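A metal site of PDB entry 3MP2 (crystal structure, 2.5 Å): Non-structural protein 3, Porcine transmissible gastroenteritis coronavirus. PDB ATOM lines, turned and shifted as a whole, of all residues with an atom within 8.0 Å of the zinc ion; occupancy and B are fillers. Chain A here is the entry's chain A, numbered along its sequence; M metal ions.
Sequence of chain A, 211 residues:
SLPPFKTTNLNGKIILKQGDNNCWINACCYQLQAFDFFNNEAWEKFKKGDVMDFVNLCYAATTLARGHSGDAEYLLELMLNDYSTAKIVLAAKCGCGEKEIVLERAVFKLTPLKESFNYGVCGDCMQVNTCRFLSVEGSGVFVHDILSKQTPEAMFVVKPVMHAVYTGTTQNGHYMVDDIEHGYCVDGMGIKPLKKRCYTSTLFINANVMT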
ATOM      1  N   ALA A  92     -21.597  28.878  -1.928  1.00  0.00           N
ATOM      2  CA  ALA A  92     -22.319  28.164  -0.902  1.00  0.00           C
ATOM      3  C   ALA A  92     -23.345  27.161  -1.481  1.00  0.00           C
ATOM      4  O   ALA A  92     -24.336  27.528  -2.156  1.00  0.00           O
ATOM      5  CB  ALA A  92     -22.981  29.149   0.000  1.00  0.00           C
ATOM      6  N   LYS A  93     -23.084  25.899  -1.204  1.00  0.00           N
ATOM      7  CA  LYS A  93     -23.883  24.804  -1.696  1.00  0.00           C
ATOM      8  C   LYS A  93     -24.806  24.343  -0.604  1.00  0.00           C
ATOM      9  O   LYS A  93     -24.363  24.134   0.488  1.00  0.00           O
ATOM     10  CB  LYS A  93     -22.933  23.679  -2.059  1.00  0.00           C
ATOM     11  CG  LYS A  93     -23.455  22.621  -3.005  1.00  0.00           C
ATOM     12  CD  LYS A  93     -22.282  21.644  -3.414  1.00  0.00           C
ATOM     13  CE  LYS A  93     -21.391  22.202  -4.579  1.00  0.00           C
ATOM     14  NZ  LYS A  93     -21.801  21.681  -5.964  1.00  0.00           N
ATOM     15  N   CYS A  94     -26.108  24.219  -0.892  1.00  0.00           N
ATOM     16  CA  CYS A  94     -27.038  23.511  -0.008  1.00  0.00           C
ATOM     17  C   CYS A  94     -28.024  22.650  -0.816  1.00  0.00           C
ATOM     18  O   CYS A  94     -27.763  22.316  -1.955  1.00  0.00           O
ATOM     19  CB  CYS A  94     -27.811  24.529   0.802  1.00  0.00           C
ATOM     20  SG  CYS A  94     -28.856  25.523  -0.241  1.00  0.00           S
ATOM     21  N   GLY A  95     -29.196  22.321  -0.274  1.00  0.00           N
ATOM     22  CA  GLY A  95     -30.118  21.479  -1.023  1.00  0.00           C
ATOM     23  C   GLY A  95     -30.911  22.264  -2.096  1.00  0.00           C
ATOM     24  O   GLY A  95     -31.680  21.689  -2.849  1.00  0.00           O
ATOM     25  N   CYS A  96     -30.761  23.589  -2.122  1.00  0.00           N
ATOM     26  CA  CYS A  96     -31.490  24.388  -3.101  1.00  0.00           C
ATOM     27  C   CYS A  96     -30.663  24.561  -4.377  1.00  0.00           C
ATOM     28  O   CYS A  96     -31.231  24.802  -5.447  1.00  0.00           O
ATOM     29  CB  CYS A  96     -31.899  25.759  -2.541  1.00  0.00           C
ATOM     30  SG  CYS A  96     -32.789  25.547  -0.995  1.00  0.00           S
ATOM     31  N   GLY A  97     -29.337  24.430  -4.242  1.00  0.00           N
ATOM     32  CA  GLY A  97     -28.432  24.784  -5.334  1.00  0.00           C
ATOM     33  C   GLY A  97     -27.165  25.408  -4.797  1.00  0.00           C
ATOM     34  O   GLY A  97     -26.713  25.082  -3.708  1.00  0.00           O
ATOM     35  N   GLU A  98     -26.575  26.309  -5.595  1.00  0.00           N
ATOM     36  CA  GLU A  98     -25.338  26.967  -5.250  1.00  0.00           C
ATOM     37  C   GLU A  98     -25.490  28.471  -5.389  1.00  0.00           C
ATOM     38  O   GLU A  98     -26.070  28.922  -6.341  1.00  0.00           O
ATOM     39  CB  GLU A  98     -24.157  26.476  -6.087  1.00  0.00           C
ATOM     40  CG  GLU A  98     -22.856  26.850  -5.392  1.00  0.00           C
ATOM     41  CD  GLU A  98     -21.553  26.537  -6.183  1.00  0.00           C
ATOM     42  OE1 GLU A  98     -21.286  27.261  -7.196  1.00  0.00           O
ATOM     43  OE2 GLU A  98     -20.786  25.607  -5.754  1.00  0.00           O
ATOM     44  N   LYS A  99     -25.010  29.243  -4.426  1.00  0.00           N
ATOM     45  CA  LYS A  99     -25.146  30.669  -4.521  1.00  0.00           C
ATOM     46  C   LYS A  99     -23.900  31.348  -3.957  1.00  0.00           C
ATOM     47  O   LYS A  99     -23.049  30.707  -3.386  1.00  0.00           O
ATOM     48  CB  LYS A  99     -26.435  31.150  -3.838  1.00  0.00           C
ATOM     49  CG  LYS A  99     -26.215  31.293  -2.378  1.00  0.00           C
ATOM     50  CD  LYS A  99     -27.372  31.038  -1.492  1.00  0.00           C
ATOM     51  CE  LYS A  99     -26.792  30.656  -0.033  1.00  0.00           C
ATOM     52  NZ  LYS A  99     -27.326  29.300   0.612  1.00  0.00           N
ATOM     53  N   VAL A 121     -26.625  28.221   7.725  1.00  0.00           N
ATOM     54  CA  VAL A 121     -27.581  27.246   7.254  1.00  0.00           C
ATOM     55  C   VAL A 121     -28.508  27.969   6.308  1.00  0.00           C
ATOM     56  O   VAL A 121     -28.859  29.114   6.548  1.00  0.00           O
ATOM     57  CB  VAL A 121     -28.528  26.749   8.364  1.00  0.00           C
ATOM     58  CG1 VAL A 121     -27.797  26.006   9.375  1.00  0.00           C
ATOM     59  CG2 VAL A 121     -29.196  27.963   8.964  1.00  0.00           C
ATOM     60  N   CYS A 122     -28.953  27.271   5.296  1.00  0.00           N
ATOM     61  CA  CYS A 122     -29.891  27.847   4.358  1.00  0.00           C
ATOM     62  C   CYS A 122     -31.260  27.785   4.952  1.00  0.00           C
ATOM     63  O   CYS A 122     -31.716  26.730   5.363  1.00  0.00           O
ATOM     64  CB  CYS A 122     -29.789  27.148   3.007  1.00  0.00           C
ATOM     65  SG  CYS A 122     -31.253  27.444   1.993  1.00  0.00           S
ATOM     66  N   GLY A 123     -31.933  28.922   5.024  1.00  0.00           N
ATOM     67  CA  GLY A 123     -33.264  28.989   5.616  1.00  0.00           C
ATOM     68  C   GLY A 123     -34.377  28.332   4.800  1.00  0.00           C
ATOM     69  O   GLY A 123     -35.438  28.100   5.344  1.00  0.00           O
ATOM     70  N   ASP A 124     -34.177  28.062   3.500  1.00  0.00           N
ATOM     71  CA  ASP A 124     -35.167  27.301   2.708  1.00  0.00           C
ATOM     72  C   ASP A 124     -35.001  25.757   2.778  1.00  0.00           C
ATOM     73  O   ASP A 124     -35.998  25.075   2.686  1.00  0.00           O
ATOM     74  CB  ASP A 124     -35.119  27.654   1.211  1.00  0.00           C
ATOM     75  CG  ASP A 124     -35.134  29.138   0.984  1.00  0.00           C
ATOM     76  OD1 ASP A 124     -35.954  29.793   1.652  1.00  0.00           O
ATOM     77  OD2 ASP A 124     -34.339  29.650   0.141  1.00  0.00           O
ATOM     78  N   CYS A 125     -33.798  25.190   2.838  1.00  0.00           N
ATOM     79  CA  CYS A 125     -33.787  23.773   2.934  1.00  0.00           C
ATOM     80  C   CYS A 125     -33.390  23.275   4.370  1.00  0.00           C
ATOM     81  O   CYS A 125     -33.356  22.071   4.596  1.00  0.00           O
ATOM     82  CB  CYS A 125     -32.883  23.201   1.880  1.00  0.00           C
ATOM     83  SG  CYS A 125     -31.207  23.829   2.059  1.00  0.00           S
ATOM     84  N   MET A 126     -33.049  24.229   5.264  1.00  0.00           N
ATOM     85  CA  MET A 126     -32.359  23.996   6.544  1.00  0.00           C
ATOM     86  C   MET A 126     -31.098  23.137   6.521  1.00  0.00           C
ATOM     87  O   MET A 126     -30.834  22.461   7.550  1.00  0.00           O
ATOM     88  CB  MET A 126     -33.311  23.402   7.623  1.00  0.00           C
ATOM     89  CG  MET A 126     -34.627  24.133   7.685  1.00  0.00           C
ATOM     90  SD  MET A 126     -35.784  23.675   8.971  1.00  0.00           S
ATOM     91  CE  MET A 126     -34.887  24.315  10.421  1.00  0.00           C
ATOM     92  N   GLN A 127     -30.327  23.104   5.444  1.00  0.00           N
ATOM     93  CA  GLN A 127     -29.064  22.380   5.521  1.00  0.00           C
ATOM     94  C   GLN A 127     -27.919  23.346   5.794  1.00  0.00           C
ATOM     95  O   GLN A 127     -28.063  24.520   5.527  1.00  0.00           O
ATOM     96  CB  GLN A 127     -28.797  21.626   4.245  1.00  0.00           C
ATOM     97  CG  GLN A 127     -29.868  20.606   3.920  1.00  0.00           C
ATOM     98  CD  GLN A 127     -29.665  19.951   2.552  1.00  0.00           C
ATOM     99  OE1 GLN A 127     -28.536  19.849   2.013  1.00  0.00           O
ATOM    100  NE2 GLN A 127     -30.771  19.536   1.966  1.00  0.00           N
ATOM    101  N   VAL A 128     -26.762  22.881   6.284  1.00  0.00           N
ATOM    102  CA  VAL A 128     -25.621  23.796   6.447  1.00  0.00           C
ATOM    103  C   VAL A 128     -25.046  24.054   5.071  1.00  0.00           C
ATOM    104  O   VAL A 128     -25.013  23.118   4.248  1.00  0.00           O
ATOM    105  CB  VAL A 128     -24.477  23.182   7.301  1.00  0.00           C
ATOM    106  CG1 VAL A 128     -25.004  22.655   8.650  1.00  0.00           C
ATOM    107  CG2 VAL A 128     -23.796  22.061   6.488  1.00  0.00           C
ATOM    108  N   ASN A 129     -24.612  25.286   4.802  1.00  0.00           N
ATOM    109  CA  ASN A 129     -23.947  25.625   3.544  1.00  0.00           C
ATOM    110  C   ASN A 129     -22.528  25.073   3.551  1.00  0.00           C
ATOM    111  O   ASN A 129     -21.773  25.351   4.504  1.00  0.00           O
ATOM    112  CB  ASN A 129     -23.857  27.152   3.392  1.00  0.00           C
ATOM    113  CG  ASN A 129     -25.195  27.809   3.359  1.00  0.00           C
ATOM    114  OD1 ASN A 129     -26.066  27.427   2.555  1.00  0.00           O
ATOM    115  ND2 ASN A 129     -25.399  28.826   4.219  1.00  0.00           N
HETATM  116 ZN    ZN M   1     -31.050  25.622   0.569  1.00  0.00          ZN
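The backbone NH (N) of Asp 124 lies close to the side-chain sulfur (SG) of Cys 122, at 3.3 Å. O of Gln 127 lies within hydrogen-bond range of N of Cys 122, 2.9 Å away. The backbone NH of Gly 95 lies close to the side-chain sulfur of Cys 125 (3.4 Å). The side-chain sulfur (SG) of Cys 125 lies close to the backbone NH (N) of Gln 127 (3.6 Å). The side-chain amide oxygen of Gln 127 is in hydrogen-bond range of the backbone NH of Gly 95.
N of Gly 95 touches the zinc ion, 3.9 Å away. Five residues have an atom within 4 Å of the zinc ion: Cys 94, Gly 95, Cys 96, Cys 122 and Cys 125. The nearest printed residue that does not touch the zinc ion is Asp 124 (4.5 Å).
The zinc ion is bound by the side-chain sulfur (SG) of Cys 122, the side-chain sulfur (SG) of Cys 125, the side-chain sulfur (SG) of Cys 96 and the side-chain sulfur (SG) of Cys 94. The zinc ion has four donor atoms within binding distance.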
